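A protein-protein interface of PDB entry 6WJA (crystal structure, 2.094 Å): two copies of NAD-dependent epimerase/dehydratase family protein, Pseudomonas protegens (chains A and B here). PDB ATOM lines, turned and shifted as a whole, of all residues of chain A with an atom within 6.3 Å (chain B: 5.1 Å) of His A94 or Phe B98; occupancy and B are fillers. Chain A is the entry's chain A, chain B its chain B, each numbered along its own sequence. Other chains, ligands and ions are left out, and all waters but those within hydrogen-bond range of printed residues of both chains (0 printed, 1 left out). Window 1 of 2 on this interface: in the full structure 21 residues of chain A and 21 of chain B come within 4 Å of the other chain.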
ATOM      1  N   ASP A  89      17.095   2.473  -8.261  1.00  0.00           N
ATOM      2  CA  ASP A  89      18.412   3.089  -8.434  1.00  0.00           C
ATOM      3  C   ASP A  89      18.421   3.920  -9.709  1.00  0.00           C
ATOM      4  O   ASP A  89      18.978   3.514 -10.739  1.00  0.00           O
ATOM      5  CB  ASP A  89      19.507   2.021  -8.463  1.00  0.00           C
ATOM      6  CG  ASP A  89      20.890   2.608  -8.272  1.00  0.00           C
ATOM      7  OD1 ASP A  89      21.078   3.819  -8.544  1.00  0.00           O
ATOM      8  OD2 ASP A  89      21.784   1.856  -7.845  1.00  0.00           O
ATOM      9  N   PRO A  90      17.795   5.105  -9.678  1.00  0.00           N
ATOM     10  CA  PRO A  90      17.776   5.957 -10.879  1.00  0.00           C
ATOM     11  C   PRO A  90      19.158   6.303 -11.400  1.00  0.00           C
ATOM     12  O   PRO A  90      19.353   6.377 -12.621  1.00  0.00           O
ATOM     13  CB  PRO A  90      17.035   7.221 -10.405  1.00  0.00           C
ATOM     14  CG  PRO A  90      16.218   6.770  -9.231  1.00  0.00           C
ATOM     15  CD  PRO A  90      16.989   5.661  -8.575  1.00  0.00           C
ATOM     16  N   VAL A  91      20.119   6.526 -10.503  1.00  0.00           N
ATOM     17  CA  VAL A  91      21.430   7.018 -10.922  1.00  0.00           C
ATOM     18  C   VAL A  91      22.177   5.946 -11.707  1.00  0.00           C
ATOM     19  O   VAL A  91      22.708   6.211 -12.792  1.00  0.00           O
ATOM     20  CB  VAL A  91      22.233   7.510  -9.705  1.00  0.00           C
ATOM     21  CG1 VAL A  91      23.681   7.853 -10.098  1.00  0.00           C
ATOM     22  CG2 VAL A  91      21.544   8.727  -9.082  1.00  0.00           C
ATOM     23  N   ALA A  92      22.211   4.715 -11.187  1.00  0.00           N
ATOM     24  CA  ALA A  92      22.967   3.663 -11.862  1.00  0.00           C
ATOM     25  C   ALA A  92      22.311   3.258 -13.180  1.00  0.00           C
ATOM     26  O   ALA A  92      23.004   3.065 -14.185  1.00  0.00           O
ATOM     27  CB  ALA A  92      23.137   2.451 -10.936  1.00  0.00           C
ATOM     28  N   THR A  93      20.978   3.146 -13.210  1.00  0.00           N
ATOM     29  CA  THR A  93      20.304   2.717 -14.437  1.00  0.00           C
ATOM     30  C   THR A  93      20.320   3.800 -15.518  1.00  0.00           C
ATOM     31  O   THR A  93      20.286   3.474 -16.709  1.00  0.00           O
ATOM     32  CB  THR A  93      18.857   2.280 -14.153  1.00  0.00           C
ATOM     33  OG1 THR A  93      18.110   3.357 -13.565  1.00  0.00           O
ATOM     34  CG2 THR A  93      18.832   1.049 -13.229  1.00  0.00           C
ATOM     35  N   HIS A  94      20.372   5.082 -15.138  1.00  0.00           N
ATOM     36  CA  HIS A  94      20.498   6.127 -16.148  1.00  0.00           C
ATOM     37  C   HIS A  94      21.770   5.960 -16.976  1.00  0.00           C
ATOM     38  O   HIS A  94      21.770   6.270 -18.172  1.00  0.00           O
ATOM     39  CB  HIS A  94      20.470   7.510 -15.503  1.00  0.00           C
ATOM     40  CG  HIS A  94      20.639   8.628 -16.483  1.00  0.00           C
ATOM     41  ND1 HIS A  94      19.628   9.039 -17.331  1.00  0.00           N
ATOM     42  CD2 HIS A  94      21.707   9.418 -16.760  1.00  0.00           C
ATOM     43  CE1 HIS A  94      20.061  10.045 -18.075  1.00  0.00           C
ATOM     44  NE2 HIS A  94      21.318  10.293 -17.748  1.00  0.00           N
ATOM     45  N   GLN A  95      22.855   5.467 -16.369  1.00  0.00           N
ATOM     46  CA  GLN A  95      24.066   5.178 -17.136  1.00  0.00           C
ATOM     47  C   GLN A  95      23.795   4.147 -18.222  1.00  0.00           C
ATOM     48  O   GLN A  95      24.236   4.304 -19.366  1.00  0.00           O
ATOM     49  CB  GLN A  95      25.188   4.671 -16.214  1.00  0.00           C
ATOM     50  CG  GLN A  95      25.705   5.697 -15.238  1.00  0.00           C
ATOM     51  CD  GLN A  95      26.327   6.897 -15.930  1.00  0.00           C
ATOM     52  OE1 GLN A  95      25.836   8.025 -15.807  1.00  0.00           O
ATOM     53  NE2 GLN A  95      27.409   6.661 -16.661  1.00  0.00           N
ATOM     54  N   SER A  96      23.097   3.063 -17.870  1.00  0.00           N
ATOM     55  CA  SER A  96      22.852   1.990 -18.829  1.00  0.00           C
ATOM     56  C   SER A  96      21.733   2.336 -19.800  1.00  0.00           C
ATOM     57  O   SER A  96      21.796   1.958 -20.976  1.00  0.00           O
ATOM     58  CB  SER A  96      22.500   0.685 -18.109  1.00  0.00           C
ATOM     59  OG  SER A  96      23.606   0.136 -17.422  1.00  0.00           O
ATOM     60  N   ASN A  97      20.692   3.029 -19.327  1.00  0.00           N
ATOM     61  CA  ASN A  97      19.482   3.234 -20.125  1.00  0.00           C
ATOM     62  C   ASN A  97      19.519   4.506 -20.962  1.00  0.00           C
ATOM     63  O   ASN A  97      18.720   4.638 -21.901  1.00  0.00           O
ATOM     64  CB  ASN A  97      18.236   3.261 -19.219  1.00  0.00           C
ATOM     65  CG  ASN A  97      18.034   1.942 -18.466  1.00  0.00           C
ATOM     66  OD1 ASN A  97      18.529   0.908 -18.897  1.00  0.00           O
ATOM     67  ND2 ASN A  97      17.315   1.980 -17.344  1.00  0.00           N
ATOM     68  N   PHE A  98      20.403   5.449 -20.647  1.00  0.00           N
ATOM     69  CA  PHE A  98      20.530   6.623 -21.499  1.00  0.00           C
ATOM     70  C   PHE A  98      21.972   6.920 -21.898  1.00  0.00           C
ATOM     71  O   PHE A  98      22.237   7.182 -23.072  1.00  0.00           O
ATOM     72  CB  PHE A  98      19.957   7.885 -20.855  1.00  0.00           C
ATOM     73  CG  PHE A  98      20.307   9.121 -21.638  1.00  0.00           C
ATOM     74  CD1 PHE A  98      19.597   9.442 -22.786  1.00  0.00           C
ATOM     75  CD2 PHE A  98      21.409   9.894 -21.297  1.00  0.00           C
ATOM     76  CE1 PHE A  98      19.932  10.541 -23.550  1.00  0.00           C
ATOM     77  CE2 PHE A  98      21.764  10.991 -22.063  1.00  0.00           C
ATOM     78  CZ  PHE A  98      21.018  11.320 -23.193  1.00  0.00           C
ATOM     79  N   ILE A  99      22.909   6.937 -20.942  1.00  0.00           N
ATOM     80  CA  ILE A  99      24.277   7.346 -21.280  1.00  0.00           C
ATOM     81  C   ILE A  99      24.855   6.426 -22.347  1.00  0.00           C
ATOM     82  O   ILE A  99      25.578   6.867 -23.252  1.00  0.00           O
ATOM     83  CB  ILE A  99      25.163   7.382 -20.019  1.00  0.00           C
ATOM     84  CG1 ILE A  99      24.614   8.409 -19.021  1.00  0.00           C
ATOM     85  CG2 ILE A  99      26.642   7.710 -20.386  1.00  0.00           C
ATOM     86  CD1 ILE A  99      24.794   9.866 -19.482  1.00  0.00           C
ATOM     87  N   ALA A 100      24.534   5.135 -22.270  1.00  0.00           N
ATOM     88  CA  ALA A 100      25.020   4.210 -23.288  1.00  0.00           C
ATOM     89  C   ALA A 100      24.542   4.625 -24.678  1.00  0.00           C
ATOM     90  O   ALA A 100      25.285   4.500 -25.657  1.00  0.00           O
ATOM     91  CB  ALA A 100      24.576   2.784 -22.961  1.00  0.00           C
ATOM     92  N   PRO A 145      12.337   6.225 -14.295  1.00  0.00           N
ATOM     93  CA  PRO A 145      13.611   6.561 -14.958  1.00  0.00           C
ATOM     94  C   PRO A 145      13.868   5.750 -16.214  1.00  0.00           C
ATOM     95  O   PRO A 145      14.380   6.298 -17.200  1.00  0.00           O
ATOM     96  CB  PRO A 145      14.661   6.266 -13.873  1.00  0.00           C
ATOM     97  CG  PRO A 145      13.929   6.418 -12.574  1.00  0.00           C
ATOM     98  CD  PRO A 145      12.506   5.988 -12.844  1.00  0.00           C
ATOM     99  N   ASP A 149      14.336   7.509 -19.791  1.00  0.00           N
ATOM    100  CA  ASP A 149      15.611   7.294 -20.476  1.00  0.00           C
ATOM    101  C   ASP A 149      15.417   6.761 -21.894  1.00  0.00           C
ATOM    102  O   ASP A 149      16.166   7.128 -22.807  1.00  0.00           O
ATOM    103  CB  ASP A 149      16.483   6.324 -19.669  1.00  0.00           C
ATOM    104  CG  ASP A 149      17.083   6.976 -18.415  1.00  0.00           C
ATOM    105  OD1 ASP A 149      16.968   8.212 -18.237  1.00  0.00           O
ATOM    106  OD2 ASP A 149      17.666   6.245 -17.602  1.00  0.00           O
ATOM    107  N   ALA A 152      14.277   9.828 -23.821  1.00  0.00           N
ATOM    108  CA  ALA A 152      15.410  10.735 -24.015  1.00  0.00           C
ATOM    109  C   ALA A 152      16.390  10.176 -25.044  1.00  0.00           C
ATOM    110  O   ALA A 152      16.937  10.924 -25.865  1.00  0.00           O
ATOM    111  CB  ALA A 152      16.124  10.993 -22.687  1.00  0.00           C
ATOM    112  N   THR B  93      27.483  18.960 -21.521  1.00  0.00           N
ATOM    113  CA  THR B  93      26.336  19.739 -21.072  1.00  0.00           C
ATOM    114  C   THR B  93      25.260  18.856 -20.460  1.00  0.00           C
ATOM    115  O   THR B  93      24.498  19.329 -19.611  1.00  0.00           O
ATOM    116  CB  THR B  93      25.763  20.592 -22.211  1.00  0.00           C
ATOM    117  OG1 THR B  93      25.399  19.772 -23.324  1.00  0.00           O
ATOM    118  CG2 THR B  93      26.786  21.656 -22.664  1.00  0.00           C
ATOM    119  N   HIS B  94      25.188  17.578 -20.854  1.00  0.00           N
ATOM    120  CA  HIS B  94      24.219  16.677 -20.231  1.00  0.00           C
ATOM    121  C   HIS B  94      24.450  16.548 -18.726  1.00  0.00           C
ATOM    122  O   HIS B  94      23.487  16.399 -17.963  1.00  0.00           O
ATOM    123  CB  HIS B  94      24.264  15.299 -20.894  1.00  0.00           C
ATOM    124  CG  HIS B  94      23.319  14.313 -20.286  1.00  0.00           C
ATOM    125  ND1 HIS B  94      21.961  14.349 -20.513  1.00  0.00           N
ATOM    126  CD2 HIS B  94      23.535  13.268 -19.450  1.00  0.00           C
ATOM    127  CE1 HIS B  94      21.377  13.367 -19.848  1.00  0.00           C
ATOM    128  NE2 HIS B  94      22.311  12.697 -19.190  1.00  0.00           N
ATOM    129  N   GLN B  95      25.713  16.609 -18.288  1.00  0.00           N
ATOM    130  CA  GLN B  95      26.029  16.658 -16.862  1.00  0.00           C
ATOM    131  C   GLN B  95      25.357  17.842 -16.187  1.00  0.00           C
ATOM    132  O   GLN B  95      24.727  17.695 -15.134  1.00  0.00           O
ATOM    133  CB  GLN B  95      27.550  16.756 -16.661  1.00  0.00           C
ATOM    134  CG  GLN B  95      28.304  15.538 -17.132  1.00  0.00           C
ATOM    135  CD  GLN B  95      27.883  14.299 -16.366  1.00  0.00           C
ATOM    136  OE1 GLN B  95      27.969  14.263 -15.142  1.00  0.00           O
ATOM    137  NE2 GLN B  95      27.406  13.289 -17.082  1.00  0.00           N
ATOM    138  N   SER B  96      25.518  19.040 -16.764  1.00  0.00           N
ATOM    139  CA  SER B  96      24.960  20.245 -16.160  1.00  0.00           C
ATOM    140  C   SER B  96      23.451  20.346 -16.368  1.00  0.00           C
ATOM    141  O   SER B  96      22.734  20.833 -15.484  1.00  0.00           O
ATOM    142  CB  SER B  96      25.654  21.483 -16.726  1.00  0.00           C
ATOM    143  OG  SER B  96      27.019  21.537 -16.314  1.00  0.00           O
ATOM    144  N   ASN B  97      22.948  19.909 -17.527  1.00  0.00           N
ATOM    145  CA  ASN B  97      21.551  20.153 -17.881  1.00  0.00           C
ATOM    146  C   ASN B  97      20.600  19.053 -17.426  1.00  0.00           C
ATOM    147  O   ASN B  97      19.379  19.279 -17.402  1.00  0.00           O
ATOM    148  CB  ASN B  97      21.419  20.340 -19.394  1.00  0.00           C
ATOM    149  CG  ASN B  97      22.166  21.564 -19.884  1.00  0.00           C
ATOM    150  OD1 ASN B  97      22.515  22.441 -19.091  1.00  0.00           O
ATOM    151  ND2 ASN B  97      22.423  21.625 -21.183  1.00  0.00           N
ATOM    152  N   PHE B  98      21.115  17.872 -17.076  1.00  0.00           N
ATOM    153  CA  PHE B  98      20.249  16.817 -16.564  1.00  0.00           C
ATOM    154  C   PHE B  98      20.781  16.152 -15.298  1.00  0.00           C
ATOM    155  O   PHE B  98      20.023  15.966 -14.342  1.00  0.00           O
ATOM    156  CB  PHE B  98      20.002  15.705 -17.583  1.00  0.00           C
ATOM    157  CG  PHE B  98      19.288  14.537 -16.967  1.00  0.00           C
ATOM    158  CD1 PHE B  98      17.928  14.605 -16.736  1.00  0.00           C
ATOM    159  CD2 PHE B  98      19.991  13.429 -16.504  1.00  0.00           C
ATOM    160  CE1 PHE B  98      17.259  13.566 -16.114  1.00  0.00           C
ATOM    161  CE2 PHE B  98      19.336  12.399 -15.862  1.00  0.00           C
ATOM    162  CZ  PHE B  98      17.969  12.458 -15.677  1.00  0.00           C
ATOM    163  N   ILE B  99      22.052  15.732 -15.298  1.00  0.00           N
ATOM    164  CA  ILE B  99      22.591  15.001 -14.147  1.00  0.00           C
ATOM    165  C   ILE B  99      22.446  15.830 -12.876  1.00  0.00           C
ATOM    166  O   ILE B  99      22.075  15.310 -11.818  1.00  0.00           O
ATOM    167  CB  ILE B  99      24.055  14.596 -14.404  1.00  0.00           C
ATOM    168  CG1 ILE B  99      24.150  13.699 -15.658  1.00  0.00           C
ATOM    169  CG2 ILE B  99      24.659  13.925 -13.164  1.00  0.00           C
ATOM    170  CD1 ILE B  99      23.643  12.269 -15.478  1.00  0.00           C
ATOM    171  N   ALA B 100      22.699  17.142 -12.968  1.00  0.00           N
ATOM    172  CA  ALA B 100      22.517  18.018 -11.813  1.00  0.00           C
ATOM    173  C   ALA B 100      21.099  17.924 -11.249  1.00  0.00           C
ATOM    174  O   ALA B 100      20.907  17.932 -10.030  1.00  0.00           O
ATOM    175  CB  ALA B 100      22.829  19.460 -12.205  1.00  0.00           C
ATOM    176  N   THR B 101      20.091  17.846 -12.122  1.00  0.00           N
ATOM    177  CA  THR B 101      18.721  17.677 -11.644  1.00  0.00           C
ATOM    178  C   THR B 101      18.555  16.339 -10.935  1.00  0.00           C
ATOM    179  O   THR B 101      17.977  16.266  -9.843  1.00  0.00           O
ATOM    180  CB  THR B 101      17.736  17.775 -12.808  1.00  0.00           C
ATOM    181  OG1 THR B 101      17.850  19.064 -13.430  1.00  0.00           O
ATOM    182  CG2 THR B 101      16.322  17.564 -12.309  1.00  0.00           C
ATOM    183  N   LEU B 102      19.051  15.265 -11.550  1.00  0.00           N
ATOM    184  CA  LEU B 102      18.944  13.941 -10.943  1.00  0.00           C
ATOM    185  C   LEU B 102      19.632  13.901  -9.579  1.00  0.00           C
ATOM    186  O   LEU B 102      19.065  13.403  -8.600  1.00  0.00           O
ATOM    187  CB  LEU B 102      19.537  12.890 -11.882  1.00  0.00           C
ATOM    188  CG  LEU B 102      19.670  11.471 -11.328  1.00  0.00           C
ATOM    189  CD1 LEU B 102      18.335  10.943 -10.831  1.00  0.00           C
ATOM    190  CD2 LEU B 102      20.250  10.535 -12.386  1.00  0.00           C
ATOM    191  N   ASP B 149      17.271  17.613 -22.325  1.00  0.00           N
ATOM    192  CA  ASP B 149      17.683  17.495 -20.927  1.00  0.00           C
ATOM    193  C   ASP B 149      16.731  18.238 -19.997  1.00  0.00           C
ATOM    194  O   ASP B 149      16.481  17.786 -18.875  1.00  0.00           O
ATOM    195  CB  ASP B 149      19.111  18.013 -20.748  1.00  0.00           C
ATOM    196  CG  ASP B 149      20.158  17.041 -21.291  1.00  0.00           C
ATOM    197  OD1 ASP B 149      19.799  15.911 -21.704  1.00  0.00           O
ATOM    198  OD2 ASP B 149      21.345  17.414 -21.314  1.00  0.00           O
ATOM    199  N   ALA B 152      13.707  15.844 -19.917  1.00  0.00           N
ATOM    200  CA  ALA B 152      14.062  14.710 -19.064  1.00  0.00           C
ATOM    201  C   ALA B 152      14.064  15.108 -17.597  1.00  0.00           C
ATOM    202  O   ALA B 152      13.601  14.350 -16.736  1.00  0.00           O
ATOM    203  CB  ALA B 152      15.434  14.154 -19.461  1.00  0.00           C
ATOM    204  N   SER B 153      14.579  16.307 -17.297  1.00  0.00           N
ATOM    205  CA  SER B 153      14.545  16.819 -15.932  1.00  0.00           C
ATOM    206  C   SER B 153      13.122  16.889 -15.401  1.00  0.00           C
ATOM    207  O   SER B 153      12.879  16.541 -14.241  1.00  0.00           O
ATOM    208  CB  SER B 153      15.192  18.211 -15.860  1.00  0.00           C
ATOM    209  OG  SER B 153      16.608  18.146 -15.931  1.00  0.00           O
ATOM    210  N   TYR B 156      11.906  13.278 -14.578  1.00  0.00           N
ATOM    211  CA  TYR B 156      12.482  12.760 -13.344  1.00  0.00           C
ATOM    212  C   TYR B 156      11.913  13.470 -12.127  1.00  0.00           C
ATOM    213  O   TYR B 156      11.668  12.832 -11.097  1.00  0.00           O
ATOM    214  CB  TYR B 156      13.998  12.898 -13.377  1.00  0.00           C
ATOM    215  CG  TYR B 156      14.689  11.693 -13.946  1.00  0.00           C
ATOM    216  CD1 TYR B 156      14.606  11.396 -15.303  1.00  0.00           C
ATOM    217  CD2 TYR B 156      15.443  10.852 -13.126  1.00  0.00           C
ATOM    218  CE1 TYR B 156      15.253  10.278 -15.832  1.00  0.00           C
ATOM    219  CE2 TYR B 156      16.103   9.739 -13.646  1.00  0.00           C
ATOM    220  CZ  TYR B 156      16.003   9.459 -14.997  1.00  0.00           C
ATOM    221  OH  TYR B 156      16.649   8.364 -15.523  1.00  0.00           O
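O of Pro A90 sits at hydrogen-bond distance from OG1 of Thr A93 (3.4 Å). The side-chain carboxylate of Asp A149 sits at hydrogen-bond distance from a ring nitrogen (ND1) of His A94 (2.9 Å). The backbone carbonyl oxygen of His A94 is in hydrogen-bond range of the backbone NH of Ile A99 (3.1 Å). The side-chain carboxylate (OD1) of Asp B149 is in hydrogen-bond range of a ring nitrogen (ND1) of His B94 (2.9 Å). The backbone carbonyl oxygen of His B94 sits at hydrogen-bond distance from the backbone NH of Ile B99 (3.1 Å). The backbone NH of Val A91 sits close to the side-chain carboxylate of Asp A89.
His B94 touches its own counterpart, His A94. His A94 touches Phe B98, and with the chains exchanged Phe A98 touches His B94. His A94 touches Ile B99, and with the chains exchanged Ile A99 touches His B94. Positions printed for both chains: 93, 94, 95, 96, 97, 98, 99, 100, 149 and 152. Of the 10 pairs that touch across the chains among the printed residues, 5 have their exchanged pair printed and touching as well.
Of the 14 printed residues of chain B, 5 touch a printed residue of chain A. Hydrophobic or aromatic side chains of chain B within 4 Å of the printed part of chain A: His B94, Phe B98, Ile B99, Leu B102 and Tyr B156. Among the printed residues, no Asp or Glu carboxylate lies within 4 Å of a Lys or Arg side-chain nitrogen of the other chain.
A ring nitrogen (NE2) of His B94 lies within hydrogen-bond range of a ring nitrogen (NE2) of His A94 (3.0 Å). O of Pro A145 lies close to OH of Tyr B156 (3.5 Å). The side-chain carboxylate of Asp A149 is in hydrogen-bond range of the side-chain hydroxyl of Tyr B156.
Of chain B, only His B94 (3.0 Å), Phe B98 (3.3 Å), Ile B99 (3.7 Å) and Tyr B156 (3.5 Å) come within 4 Å of His A94. Of chain A, only His A94 comes within 4 Å of Phe B98. Of the printed residues of chain B, Phe A98 touches His B94 (3.3 Å). Printed residues of chain B within 4 Å of Pro A90: Leu B102. Printed residues of chain A within 4 Å of Tyr B156: His A94 (3.5 Å), Pro A145 (3.3 Å) and Asp A149 (2.7 Å). Printed residues of chain B within 4 Å of Asp A149: Tyr B156 (2.7 Å). The nearest residue of chain A that does not touch Phe B98 is Asp A149 (5.1 Å). The nearest printed residue of chain B that does not touch Phe A98 is Asp B149 (5.0 Å).
Among the printed residues, merely in contact across the chains: Phe A98 with His B94 (3.3 Å), His A94 with Phe B98 (3.3 Å), His A94 with Tyr B156 (3.5 Å), Ile A99 with His B94 (3.6 Å), His A94 with Ile B99 (3.7 Å), Pro A90 with Leu B102 (3.97 Å) and Val A91 with Leu B102 (3.98 Å).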
